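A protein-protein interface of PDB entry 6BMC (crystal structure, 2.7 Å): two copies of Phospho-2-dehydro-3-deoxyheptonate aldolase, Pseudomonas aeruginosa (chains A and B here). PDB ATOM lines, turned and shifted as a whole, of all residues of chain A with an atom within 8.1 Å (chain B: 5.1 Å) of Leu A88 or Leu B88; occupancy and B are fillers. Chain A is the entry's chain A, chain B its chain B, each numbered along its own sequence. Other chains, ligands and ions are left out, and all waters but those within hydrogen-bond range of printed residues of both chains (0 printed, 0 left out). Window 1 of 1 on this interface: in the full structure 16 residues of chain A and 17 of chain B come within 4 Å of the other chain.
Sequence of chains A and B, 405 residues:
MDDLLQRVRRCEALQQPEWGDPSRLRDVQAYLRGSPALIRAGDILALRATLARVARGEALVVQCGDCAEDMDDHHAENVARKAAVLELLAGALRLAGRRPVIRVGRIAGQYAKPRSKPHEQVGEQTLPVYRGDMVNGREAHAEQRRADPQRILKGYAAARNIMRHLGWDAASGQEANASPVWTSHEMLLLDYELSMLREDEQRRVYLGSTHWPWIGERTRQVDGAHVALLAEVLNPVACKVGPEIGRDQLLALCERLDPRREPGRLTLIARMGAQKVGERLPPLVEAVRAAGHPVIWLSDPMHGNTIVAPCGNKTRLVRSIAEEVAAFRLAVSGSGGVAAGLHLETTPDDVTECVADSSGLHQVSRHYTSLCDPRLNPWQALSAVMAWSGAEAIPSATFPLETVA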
ATOM      1  N   VAL A  62      -3.913 -11.480  -0.663  1.00  0.00           N
ATOM      2  CA  VAL A  62      -4.143 -10.698  -1.872  1.00  0.00           C
ATOM      3  C   VAL A  62      -5.362 -11.229  -2.611  1.00  0.00           C
ATOM      4  O   VAL A  62      -5.327 -12.327  -3.168  1.00  0.00           O
ATOM      5  CB  VAL A  62      -2.944 -10.768  -2.831  1.00  0.00           C
ATOM      6  CG1 VAL A  62      -3.252 -10.019  -4.117  1.00  0.00           C
ATOM      7  CG2 VAL A  62      -1.706 -10.198  -2.165  1.00  0.00           C
ATOM      8  N   ARG A  81      -2.899 -16.319 -17.073  1.00  0.00           N
ATOM      9  CA  ARG A  81      -2.421 -14.944 -16.980  1.00  0.00           C
ATOM     10  C   ARG A  81      -2.918 -14.268 -15.703  1.00  0.00           C
ATOM     11  O   ARG A  81      -2.148 -13.598 -15.012  1.00  0.00           O
ATOM     12  CB  ARG A  81      -2.840 -14.145 -18.220  1.00  0.00           C
ATOM     13  CG  ARG A  81      -2.422 -14.788 -19.547  1.00  0.00           C
ATOM     14  CD  ARG A  81      -2.004 -13.769 -20.608  1.00  0.00           C
ATOM     15  NE  ARG A  81      -3.074 -12.820 -20.922  1.00  0.00           N
ATOM     16  CZ  ARG A  81      -2.929 -11.496 -20.935  1.00  0.00           C
ATOM     17  NH1 ARG A  81      -1.747 -10.948 -20.669  1.00  0.00           N
ATOM     18  NH2 ARG A  81      -3.957 -10.715 -21.239  1.00  0.00           N
ATOM     19  N   LYS A  82      -4.173 -14.518 -15.346  1.00  0.00           N
ATOM     20  CA  LYS A  82      -4.726 -14.000 -14.098  1.00  0.00           C
ATOM     21  C   LYS A  82      -4.001 -14.564 -12.874  1.00  0.00           C
ATOM     22  O   LYS A  82      -3.744 -13.841 -11.907  1.00  0.00           O
ATOM     23  CB  LYS A  82      -6.216 -14.317 -14.003  1.00  0.00           C
ATOM     24  CG  LYS A  82      -7.077 -13.543 -14.985  1.00  0.00           C
ATOM     25  CD  LYS A  82      -8.529 -13.980 -14.884  1.00  0.00           C
ATOM     26  CE  LYS A  82      -9.384 -13.367 -15.979  1.00  0.00           C
ATOM     27  NZ  LYS A  82     -10.820 -13.747 -15.833  1.00  0.00           N
ATOM     28  N   ALA A  83      -3.674 -15.855 -12.922  1.00  0.00           N
ATOM     29  CA  ALA A  83      -2.935 -16.505 -11.837  1.00  0.00           C
ATOM     30  C   ALA A  83      -1.510 -15.962 -11.731  1.00  0.00           C
ATOM     31  O   ALA A  83      -0.956 -15.852 -10.637  1.00  0.00           O
ATOM     32  CB  ALA A  83      -2.908 -18.010 -12.046  1.00  0.00           C
ATOM     33  N   ALA A  84      -0.930 -15.615 -12.872  1.00  0.00           N
ATOM     34  CA  ALA A  84       0.392 -15.002 -12.903  1.00  0.00           C
ATOM     35  C   ALA A  84       0.389 -13.623 -12.254  1.00  0.00           C
ATOM     36  O   ALA A  84       1.357 -13.235 -11.597  1.00  0.00           O
ATOM     37  CB  ALA A  84       0.880 -14.895 -14.337  1.00  0.00           C
ATOM     38  N   VAL A  85      -0.673 -12.860 -12.490  1.00  0.00           N
ATOM     39  CA  VAL A  85      -0.851 -11.587 -11.808  1.00  0.00           C
ATOM     40  C   VAL A  85      -0.825 -11.818 -10.302  1.00  0.00           C
ATOM     41  O   VAL A  85      -0.154 -11.091  -9.571  1.00  0.00           O
ATOM     42  CB  VAL A  85      -2.172 -10.898 -12.213  1.00  0.00           C
ATOM     43  CG1 VAL A  85      -2.488  -9.748 -11.270  1.00  0.00           C
ATOM     44  CG2 VAL A  85      -2.093 -10.398 -13.650  1.00  0.00           C
ATOM     45  N   LEU A  86      -1.512 -12.866  -9.855  1.00  0.00           N
ATOM     46  CA  LEU A  86      -1.540 -13.210  -8.435  1.00  0.00           C
ATOM     47  C   LEU A  86      -0.158 -13.601  -7.919  1.00  0.00           C
ATOM     48  O   LEU A  86       0.230 -13.196  -6.826  1.00  0.00           O
ATOM     49  CB  LEU A  86      -2.545 -14.334  -8.163  1.00  0.00           C
ATOM     50  CG  LEU A  86      -3.958 -13.856  -7.818  1.00  0.00           C
ATOM     51  CD1 LEU A  86      -4.980 -14.954  -8.054  1.00  0.00           C
ATOM     52  CD2 LEU A  86      -4.023 -13.369  -6.379  1.00  0.00           C
ATOM     53  N   GLU A  87       0.588 -14.371  -8.710  1.00  0.00           N
ATOM     54  CA  GLU A  87       1.984 -14.669  -8.384  1.00  0.00           C
ATOM     55  C   GLU A  87       2.743 -13.375  -8.118  1.00  0.00           C
ATOM     56  O   GLU A  87       3.387 -13.219  -7.081  1.00  0.00           O
ATOM     57  CB  GLU A  87       2.667 -15.431  -9.527  1.00  0.00           C
ATOM     58  CG  GLU A  87       2.211 -16.875  -9.703  1.00  0.00           C
ATOM     59  CD  GLU A  87       2.898 -17.573 -10.868  1.00  0.00           C
ATOM     60  OE1 GLU A  87       4.139 -17.461 -10.981  1.00  0.00           O
ATOM     61  OE2 GLU A  87       2.202 -18.240 -11.671  1.00  0.00           O
ATOM     62  N   LEU A  88       2.626 -12.438  -9.052  1.00  0.00           N
ATOM     63  CA  LEU A  88       3.380 -11.192  -9.009  1.00  0.00           C
ATOM     64  C   LEU A  88       3.090 -10.406  -7.732  1.00  0.00           C
ATOM     65  O   LEU A  88       4.009  -9.949  -7.050  1.00  0.00           O
ATOM     66  CB  LEU A  88       3.046 -10.344 -10.242  1.00  0.00           C
ATOM     67  CG  LEU A  88       3.950  -9.133 -10.481  1.00  0.00           C
ATOM     68  CD1 LEU A  88       3.822  -8.650 -11.914  1.00  0.00           C
ATOM     69  CD2 LEU A  88       3.638  -8.004  -9.511  1.00  0.00           C
ATOM     70  N   LEU A  89       1.809 -10.233  -7.419  1.00  0.00           N
ATOM     71  CA  LEU A  89       1.413  -9.430  -6.267  1.00  0.00           C
ATOM     72  C   LEU A  89       1.712 -10.159  -4.960  1.00  0.00           C
ATOM     73  O   LEU A  89       2.123  -9.540  -3.976  1.00  0.00           O
ATOM     74  CB  LEU A  89      -0.070  -9.060  -6.349  1.00  0.00           C
ATOM     75  CG  LEU A  89      -0.511  -8.297  -7.606  1.00  0.00           C
ATOM     76  CD1 LEU A  89      -2.000  -7.989  -7.563  1.00  0.00           C
ATOM     77  CD2 LEU A  89       0.279  -7.013  -7.782  1.00  0.00           C
ATOM     78  N   ALA A  90       1.560 -11.481  -4.977  1.00  0.00           N
ATOM     79  CA  ALA A  90       1.843 -12.301  -3.803  1.00  0.00           C
ATOM     80  C   ALA A  90       3.306 -12.192  -3.395  1.00  0.00           C
ATOM     81  O   ALA A  90       3.619 -11.993  -2.220  1.00  0.00           O
ATOM     82  CB  ALA A  90       1.485 -13.749  -4.076  1.00  0.00           C
ATOM     83  N   GLY A  91       4.198 -12.338  -4.369  1.00  0.00           N
ATOM     84  CA  GLY A  91       5.626 -12.158  -4.130  1.00  0.00           C
ATOM     85  C   GLY A  91       5.937 -10.771  -3.602  1.00  0.00           C
ATOM     86  O   GLY A  91       6.669 -10.617  -2.619  1.00  0.00           O
ATOM     87  N   ALA A  92       5.340  -9.761  -4.231  1.00  0.00           N
ATOM     88  CA  ALA A  92       5.569  -8.373  -3.842  1.00  0.00           C
ATOM     89  C   ALA A  92       5.128  -8.141  -2.403  1.00  0.00           C
ATOM     90  O   ALA A  92       5.886  -7.600  -1.594  1.00  0.00           O
ATOM     91  CB  ALA A  92       4.828  -7.434  -4.776  1.00  0.00           C
ATOM     92  N   LEU A  93       3.920  -8.594  -2.078  1.00  0.00           N
ATOM     93  CA  LEU A  93       3.379  -8.406  -0.736  1.00  0.00           C
ATOM     94  C   LEU A  93       4.214  -9.142   0.305  1.00  0.00           C
ATOM     95  O   LEU A  93       4.477  -8.619   1.388  1.00  0.00           O
ATOM     96  CB  LEU A  93       1.929  -8.883  -0.663  1.00  0.00           C
ATOM     97  CG  LEU A  93       1.222  -8.609   0.670  1.00  0.00           C
ATOM     98  CD1 LEU A  93       1.244  -7.127   1.014  1.00  0.00           C
ATOM     99  CD2 LEU A  93      -0.206  -9.126   0.639  1.00  0.00           C
ATOM    100  N   ARG A  94       4.646 -10.350  -0.033  1.00  0.00           N
ATOM    101  CA  ARG A  94       5.491 -11.126   0.866  1.00  0.00           C
ATOM    102  C   ARG A  94       6.753 -10.337   1.230  1.00  0.00           C
ATOM    103  O   ARG A  94       7.156 -10.289   2.393  1.00  0.00           O
ATOM    104  CB  ARG A  94       5.842 -12.474   0.223  1.00  0.00           C
ATOM    105  CG  ARG A  94       7.031 -13.192   0.826  1.00  0.00           C
ATOM    106  CD  ARG A  94       6.642 -14.089   1.986  1.00  0.00           C
ATOM    107  NE  ARG A  94       7.507 -13.910   3.150  1.00  0.00           N
ATOM    108  CZ  ARG A  94       7.811 -14.874   4.014  1.00  0.00           C
ATOM    109  NH1 ARG A  94       7.367 -16.115   3.836  1.00  0.00           N
ATOM    110  NH2 ARG A  94       8.594 -14.601   5.048  1.00  0.00           N
ATOM    111  N   LEU A  95       7.340  -9.677   0.239  1.00  0.00           N
ATOM    112  CA  LEU A  95       8.553  -8.898   0.459  1.00  0.00           C
ATOM    113  C   LEU A  95       8.272  -7.623   1.250  1.00  0.00           C
ATOM    114  O   LEU A  95       9.044  -7.250   2.133  1.00  0.00           O
ATOM    115  CB  LEU A  95       9.209  -8.557  -0.877  1.00  0.00           C
ATOM    116  CG  LEU A  95       9.757  -9.765  -1.641  1.00  0.00           C
ATOM    117  CD1 LEU A  95      10.100  -9.381  -3.074  1.00  0.00           C
ATOM    118  CD2 LEU A  95      10.970 -10.349  -0.931  1.00  0.00           C
ATOM    119  N   ARG A 103      -3.076 -16.420  -1.877  1.00  0.00           N
ATOM    120  CA  ARG A 103      -3.619 -15.938  -3.155  1.00  0.00           C
ATOM    121  C   ARG A 103      -5.113 -16.235  -3.271  1.00  0.00           C
ATOM    122  O   ARG A 103      -5.521 -17.395  -3.267  1.00  0.00           O
ATOM    123  CB  ARG A 103      -2.901 -16.604  -4.332  1.00  0.00           C
ATOM    124  CG  ARG A 103      -1.448 -16.192  -4.519  1.00  0.00           C
ATOM    125  CD  ARG A 103      -0.701 -17.214  -5.382  1.00  0.00           C
ATOM    126  NE  ARG A 103       0.745 -17.240  -5.160  1.00  0.00           N
ATOM    127  CZ  ARG A 103       1.352 -17.807  -4.117  1.00  0.00           C
ATOM    128  NH1 ARG A 103       0.659 -18.435  -3.173  1.00  0.00           N
ATOM    129  NH2 ARG A 103       2.675 -17.760  -4.031  1.00  0.00           N
ATOM    130  N   ASN A 377      -3.852  -2.316 -14.265  1.00  0.00           N
ATOM    131  CA  ASN A 377      -2.839  -3.124 -14.923  1.00  0.00           C
ATOM    132  C   ASN A 377      -1.902  -3.697 -13.861  1.00  0.00           C
ATOM    133  O   ASN A 377      -1.742  -3.103 -12.796  1.00  0.00           O
ATOM    134  CB  ASN A 377      -2.063  -2.279 -15.940  1.00  0.00           C
ATOM    135  CG  ASN A 377      -1.313  -1.125 -15.288  1.00  0.00           C
ATOM    136  OD1 ASN A 377      -0.247  -1.316 -14.706  1.00  0.00           O
ATOM    137  ND2 ASN A 377      -1.879   0.074 -15.367  1.00  0.00           N
ATOM    138  N   PRO A 378      -1.291  -4.861 -14.141  1.00  0.00           N
ATOM    139  CA  PRO A 378      -0.466  -5.532 -13.138  1.00  0.00           C
ATOM    140  C   PRO A 378       0.556  -4.611 -12.472  1.00  0.00           C
ATOM    141  O   PRO A 378       0.718  -4.640 -11.254  1.00  0.00           O
ATOM    142  CB  PRO A 378       0.244  -6.629 -13.941  1.00  0.00           C
ATOM    143  CG  PRO A 378      -0.630  -6.856 -15.129  1.00  0.00           C
ATOM    144  CD  PRO A 378      -1.192  -5.511 -15.460  1.00  0.00           C
ATOM    145  N   TRP A 379       1.208  -3.772 -13.270  1.00  0.00           N
ATOM    146  CA  TRP A 379       2.270  -2.908 -12.767  1.00  0.00           C
ATOM    147  C   TRP A 379       1.697  -1.790 -11.891  1.00  0.00           C
ATOM    148  O   TRP A 379       2.259  -1.459 -10.847  1.00  0.00           O
ATOM    149  CB  TRP A 379       3.082  -2.341 -13.935  1.00  0.00           C
ATOM    150  CG  TRP A 379       3.184  -3.301 -15.095  1.00  0.00           C
ATOM    151  CD1 TRP A 379       2.633  -3.148 -16.333  1.00  0.00           C
ATOM    152  CD2 TRP A 379       3.785  -4.603 -15.085  1.00  0.00           C
ATOM    153  NE1 TRP A 379       2.874  -4.262 -17.101  1.00  0.00           N
ATOM    154  CE2 TRP A 379       3.579  -5.169 -16.359  1.00  0.00           C
ATOM    155  CE3 TRP A 379       4.486  -5.338 -14.128  1.00  0.00           C
ATOM    156  CZ2 TRP A 379       4.056  -6.432 -16.703  1.00  0.00           C
ATOM    157  CZ3 TRP A 379       4.955  -6.597 -14.466  1.00  0.00           C
ATOM    158  CH2 TRP A 379       4.741  -7.129 -15.746  1.00  0.00           C
ATOM    159  N   GLN A 380       0.546  -1.256 -12.281  1.00  0.00           N
ATOM    160  CA  GLN A 380      -0.171  -0.304 -11.444  1.00  0.00           C
ATOM    161  C   GLN A 380      -0.553  -0.956 -10.109  1.00  0.00           C
ATOM    162  O   GLN A 380      -0.388  -0.364  -9.038  1.00  0.00           O
ATOM    163  CB  GLN A 380      -1.421   0.193 -12.177  1.00  0.00           C
ATOM    164  N   ALA A 381      -1.023  -2.197 -10.184  1.00  0.00           N
ATOM    165  CA  ALA A 381      -1.395  -2.957  -8.994  1.00  0.00           C
ATOM    166  C   ALA A 381      -0.172  -3.215  -8.130  1.00  0.00           C
ATOM    167  O   ALA A 381      -0.236  -3.167  -6.904  1.00  0.00           O
ATOM    168  CB  ALA A 381      -2.042  -4.274  -9.394  1.00  0.00           C
ATOM    169  N   LEU A 382       0.949  -3.469  -8.791  1.00  0.00           N
ATOM    170  CA  LEU A 382       2.230  -3.598  -8.116  1.00  0.00           C
ATOM    171  C   LEU A 382       2.507  -2.363  -7.257  1.00  0.00           C
ATOM    172  O   LEU A 382       2.834  -2.488  -6.080  1.00  0.00           O
ATOM    173  CB  LEU A 382       3.332  -3.806  -9.154  1.00  0.00           C
ATOM    174  CG  LEU A 382       4.548  -4.637  -8.761  1.00  0.00           C
ATOM    175  CD1 LEU A 382       5.200  -5.186 -10.021  1.00  0.00           C
ATOM    176  CD2 LEU A 382       5.539  -3.807  -7.951  1.00  0.00           C
ATOM    177  N   SER A 383       2.316  -1.177  -7.832  1.00  0.00           N
ATOM    178  CA  SER A 383       2.479   0.072  -7.090  1.00  0.00           C
ATOM    179  C   SER A 383       1.569   0.094  -5.868  1.00  0.00           C
ATOM    180  O   SER A 383       2.010   0.404  -4.764  1.00  0.00           O
ATOM    181  CB  SER A 383       2.174   1.284  -7.979  1.00  0.00           C
ATOM    182  OG  SER A 383       2.740   1.143  -9.272  1.00  0.00           O
ATOM    183  N   VAL A 385       0.277  -2.431  -4.165  1.00  0.00           N
ATOM    184  CA  VAL A 385       0.719  -3.368  -3.129  1.00  0.00           C
ATOM    185  C   VAL A 385       1.954  -2.836  -2.413  1.00  0.00           C
ATOM    186  O   VAL A 385       2.140  -3.068  -1.225  1.00  0.00           O
ATOM    187  CB  VAL A 385       0.985  -4.797  -3.656  1.00  0.00           C
ATOM    188  CG1 VAL A 385      -0.190  -5.290  -4.486  1.00  0.00           C
ATOM    189  CG2 VAL A 385       2.282  -4.871  -4.442  1.00  0.00           C
ATOM    190  N   MET A 386       2.770  -2.085  -3.140  1.00  0.00           N
ATOM    191  CA  MET A 386       4.003  -1.543  -2.590  1.00  0.00           C
ATOM    192  C   MET A 386       3.737  -0.559  -1.458  1.00  0.00           C
ATOM    193  O   MET A 386       4.492  -0.505  -0.487  1.00  0.00           O
ATOM    194  CB  MET A 386       4.818  -0.875  -3.707  1.00  0.00           C
ATOM    195  CG  MET A 386       5.335  -1.845  -4.766  1.00  0.00           C
ATOM    196  SD  MET A 386       6.431  -3.161  -4.195  1.00  0.00           S
ATOM    197  CE  MET A 386       7.854  -2.186  -3.706  1.00  0.00           C
ATOM    198  N   ALA B  84      10.076 -16.004  -2.593  1.00  0.00           N
ATOM    199  CA  ALA B  84       9.122 -14.949  -2.916  1.00  0.00           C
ATOM    200  C   ALA B  84       9.635 -14.048  -4.036  1.00  0.00           C
ATOM    201  O   ALA B  84       8.865 -13.596  -4.878  1.00  0.00           O
ATOM    202  CB  ALA B  84       8.819 -14.122  -1.682  1.00  0.00           C
ATOM    203  N   VAL B  85      10.928 -13.749  -4.010  1.00  0.00           N
ATOM    204  CA  VAL B  85      11.557 -13.036  -5.113  1.00  0.00           C
ATOM    205  C   VAL B  85      11.338 -13.803  -6.414  1.00  0.00           C
ATOM    206  O   VAL B  85      10.959 -13.219  -7.428  1.00  0.00           O
ATOM    207  CB  VAL B  85      13.064 -12.837  -4.880  1.00  0.00           C
ATOM    208  CG1 VAL B  85      13.747 -12.375  -6.159  1.00  0.00           C
ATOM    209  CG2 VAL B  85      13.297 -11.837  -3.759  1.00  0.00           C
ATOM    210  N   LEU B  86      11.513 -15.121  -6.360  1.00  0.00           N
ATOM    211  CA  LEU B  86      11.273 -15.968  -7.524  1.00  0.00           C
ATOM    212  C   LEU B  86       9.810 -15.934  -7.971  1.00  0.00           C
ATOM    213  O   LEU B  86       9.534 -15.863  -9.165  1.00  0.00           O
ATOM    214  CB  LEU B  86      11.712 -17.409  -7.252  1.00  0.00           C
ATOM    215  CG  LEU B  86      13.166 -17.716  -7.618  1.00  0.00           C
ATOM    216  CD1 LEU B  86      13.659 -18.956  -6.890  1.00  0.00           C
ATOM    217  CD2 LEU B  86      13.315 -17.893  -9.119  1.00  0.00           C
ATOM    218  N   GLU B  87       8.879 -15.954  -7.018  1.00  0.00           N
ATOM    219  CA  GLU B  87       7.459 -15.754  -7.333  1.00  0.00           C
ATOM    220  C   GLU B  87       7.279 -14.477  -8.148  1.00  0.00           C
ATOM    221  O   GLU B  87       6.672 -14.492  -9.218  1.00  0.00           O
ATOM    222  CB  GLU B  87       6.611 -15.656  -6.059  1.00  0.00           C
ATOM    223  CG  GLU B  87       6.430 -16.959  -5.296  1.00  0.00           C
ATOM    224  CD  GLU B  87       5.616 -16.780  -4.020  1.00  0.00           C
ATOM    225  OE1 GLU B  87       4.558 -16.111  -4.075  1.00  0.00           O
ATOM    226  OE2 GLU B  87       6.017 -17.326  -2.966  1.00  0.00           O
ATOM    227  N   LEU B  88       7.838 -13.383  -7.637  1.00  0.00           N
ATOM    228  CA  LEU B  88       7.666 -12.054  -8.223  1.00  0.00           C
ATOM    229  C   LEU B  88       8.142 -12.023  -9.674  1.00  0.00           C
ATOM    230  O   LEU B  88       7.430 -11.549 -10.561  1.00  0.00           O
ATOM    231  CB  LEU B  88       8.435 -11.024  -7.385  1.00  0.00           C
ATOM    232  CG  LEU B  88       8.302  -9.522  -7.645  1.00  0.00           C
ATOM    233  CD1 LEU B  88       8.788  -9.173  -9.036  1.00  0.00           C
ATOM    234  CD2 LEU B  88       6.878  -9.034  -7.436  1.00  0.00           C
ATOM    235  N   LEU B  89       9.346 -12.526  -9.914  1.00  0.00           N
ATOM    236  CA  LEU B  89       9.932 -12.478 -11.249  1.00  0.00           C
ATOM    237  C   LEU B  89       9.252 -13.475 -12.187  1.00  0.00           C
ATOM    238  O   LEU B  89       9.058 -13.192 -13.369  1.00  0.00           O
ATOM    239  CB  LEU B  89      11.440 -12.740 -11.183  1.00  0.00           C
ATOM    240  CG  LEU B  89      12.245 -11.796 -10.277  1.00  0.00           C
ATOM    241  CD1 LEU B  89      13.720 -12.157 -10.297  1.00  0.00           C
ATOM    242  CD2 LEU B  89      12.058 -10.341 -10.678  1.00  0.00           C
ATOM    243  N   ALA B  90       8.852 -14.620 -11.642  1.00  0.00           N
ATOM    244  CA  ALA B  90       8.180 -15.651 -12.429  1.00  0.00           C
ATOM    245  C   ALA B  90       6.858 -15.133 -12.979  1.00  0.00           C
ATOM    246  O   ALA B  90       6.559 -15.303 -14.158  1.00  0.00           O
ATOM    247  CB  ALA B  90       7.942 -16.890 -11.582  1.00  0.00           C
ATOM    248  N   GLY B  91       6.070 -14.505 -12.113  1.00  0.00           N
ATOM    249  CA  GLY B  91       4.825 -13.868 -12.529  1.00  0.00           C
ATOM    250  C   GLY B  91       5.060 -12.798 -13.577  1.00  0.00           C
ATOM    251  O   GLY B  91       4.379 -12.768 -14.603  1.00  0.00           O
ATOM    252  N   ALA B  92       6.051 -11.946 -13.333  1.00  0.00           N
ATOM    253  CA  ALA B  92       6.394 -10.873 -14.263  1.00  0.00           C
ATOM    254  C   ALA B  92       6.763 -11.440 -15.629  1.00  0.00           C
ATOM    255  O   ALA B  92       6.229 -11.011 -16.649  1.00  0.00           O
ATOM    256  CB  ALA B  92       7.536 -10.032 -13.710  1.00  0.00           C
ATOM    257  N   LEU B  95       3.895 -12.866 -17.623  1.00  0.00           N
ATOM    258  CA  LEU B  95       3.089 -11.816 -18.238  1.00  0.00           C
ATOM    259  C   LEU B  95       3.791 -11.206 -19.452  1.00  0.00           C
ATOM    260  O   LEU B  95       3.155 -10.928 -20.465  1.00  0.00           O
ATOM    261  CB  LEU B  95       2.764 -10.722 -17.218  1.00  0.00           C
ATOM    262  CG  LEU B  95       1.842 -11.161 -16.081  1.00  0.00           C
ATOM    263  CD1 LEU B  95       1.832 -10.132 -14.960  1.00  0.00           C
ATOM    264  CD2 LEU B  95       0.433 -11.403 -16.600  1.00  0.00           C
ATOM    265  N   PRO B 378      14.838  -6.684  -5.507  1.00  0.00           N
ATOM    266  CA  PRO B 378      13.751  -7.326  -6.253  1.00  0.00           C
ATOM    267  C   PRO B 378      13.136  -6.413  -7.316  1.00  0.00           C
ATOM    268  O   PRO B 378      12.876  -6.852  -8.436  1.00  0.00           O
ATOM    269  CB  PRO B 378      12.722  -7.649  -5.164  1.00  0.00           C
ATOM    270  CG  PRO B 378      13.510  -7.729  -3.902  1.00  0.00           C
ATOM    271  CD  PRO B 378      14.591  -6.699  -4.055  1.00  0.00           C
ATOM    272  N   TRP B 379      12.956  -5.142  -6.973  1.00  0.00           N
ATOM    273  CA  TRP B 379      12.303  -4.193  -7.869  1.00  0.00           C
ATOM    274  C   TRP B 379      13.204  -3.850  -9.062  1.00  0.00           C
ATOM    275  O   TRP B 379      12.738  -3.760 -10.195  1.00  0.00           O
ATOM    276  CB  TRP B 379      11.919  -2.925  -7.098  1.00  0.00           C
ATOM    277  CG  TRP B 379      11.593  -3.186  -5.652  1.00  0.00           C
ATOM    278  CD1 TRP B 379      12.293  -2.755  -4.559  1.00  0.00           C
ATOM    279  CD2 TRP B 379      10.527  -3.998  -5.152  1.00  0.00           C
ATOM    280  NE1 TRP B 379      11.705  -3.219  -3.407  1.00  0.00           N
ATOM    281  CE2 TRP B 379      10.621  -3.988  -3.742  1.00  0.00           C
ATOM    282  CE3 TRP B 379       9.492  -4.727  -5.757  1.00  0.00           C
ATOM    283  CZ2 TRP B 379       9.718  -4.674  -2.928  1.00  0.00           C
ATOM    284  CZ3 TRP B 379       8.595  -5.405  -4.945  1.00  0.00           C
ATOM    285  CH2 TRP B 379       8.714  -5.373  -3.546  1.00  0.00           C
ATOM    286  N   LEU B 382      12.949  -6.752 -11.171  1.00  0.00           N
ATOM    287  CA  LEU B 382      11.677  -6.599 -11.865  1.00  0.00           C
ATOM    288  C   LEU B 382      11.870  -5.834 -13.163  1.00  0.00           C
ATOM    289  O   LEU B 382      11.433  -6.276 -14.219  1.00  0.00           O
ATOM    290  CB  LEU B 382      10.708  -5.833 -10.977  1.00  0.00           C
ATOM    291  CG  LEU B 382       9.226  -5.982 -11.263  1.00  0.00           C
ATOM    292  CD1 LEU B 382       8.470  -5.428 -10.064  1.00  0.00           C
ATOM    293  CD2 LEU B 382       8.857  -5.247 -12.541  1.00  0.00           C
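The side-chain carboxylate of Glu B87 lies within salt-bridge range of the guanidinium group of Arg A103.
Among the printed residues, merely in contact across the chains: Leu A88 with Leu B88 (3.0 Å), Met A386 with Trp B379 (3.2 Å), Arg A94 with Ala B84 (3.2 Å), Leu A382 with Leu B382 (3.3 Å), Gly A91 with Ala B84 (3.6 Å), Ala A92 with Leu B88 (3.6 Å), Ala A84 with Gly B91 (3.6 Å), Glu A87 with Gly B91 (3.7 Å), Arg A81 with Leu B95 (3.7 Å), Leu A95 with Pro B378 (3.8 Å), Gly A91 with Glu B87 (3.8 Å), Ala A90 with Glu B87 (3.9 Å), Glu A87 with Ala B90 (3.9 Å), Leu A88 with Leu B95 (3.9 Å), Leu A95 with Val B85 (3.95 Å) and Pro A378 with Leu B95 (3.98 Å).
Of chain B, only Leu B88 (3.0 Å) and Leu B95 (3.9 Å) come within 4 Å of Leu A88.
Of the printed residues of chain A, Leu B88 touches Leu A88 and Ala A92.
Printed residues of chain B within 4 Å of Leu A382: Leu B382.
Of the printed residues of chain B, Ala A84 touches Gly B91.
Printed residues of chain B within 4 Å of Arg A94: Ala B84 (3.2 Å).
Printed residues of chain B within 4 Å of Leu A95: Val B85 (3.95 Å) and Pro B378 (3.8 Å).
Ser A383 touches none of the printed residues of chain B.
The nearest residue of chain B that does not touch Leu A88 is Ala B92 (4.1 Å).
The nearest printed residue of chain A that does not touch Val B85 is Gly A91 (5.5 Å).
Hydrophobic or aromatic side chains of chain A that line the printed part of chain B: Leu A88, Ala A90, Ala A92, Leu A95, Pro A378, Leu A382 and Met A386.
Along chain A the printed residues that touch a printed residue of chain B span positions 81 to 386.
Of the 13 printed residues of chain B, 10 touch a printed residue of chain A.
Hydrophobic or aromatic side chains of chain B within 4 Å of the printed part of chain A: Ala B84, Val B85, Leu B88, Ala B90, Leu B95, Pro B378, Trp B379 and Leu B382.
Among the printed residues, Asp or Glu carboxylates within 4 Å of a Lys or Arg side-chain nitrogen of the other chain: Arg A103 with Glu B87 (2.5 Å).
Glu A87 touches Ala B90, and with the chains exchanged Ala A90 touches Glu B87.
Glu A87 touches Gly B91, and with the chains exchanged Gly A91 touches Glu B87.
Leu A88 touches its own counterpart, Leu B88.
Leu A95 touches Pro B378, and with the chains exchanged Pro A378 touches Leu B95.
Positions printed for both chains: 84, 85, 86, 87, 88, 89, 90, 91, 92, 95, 378, 379 and 382.
Of the 17 pairs that touch across the chains among the printed residues, 10 have their exchanged pair printed and touching as well.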
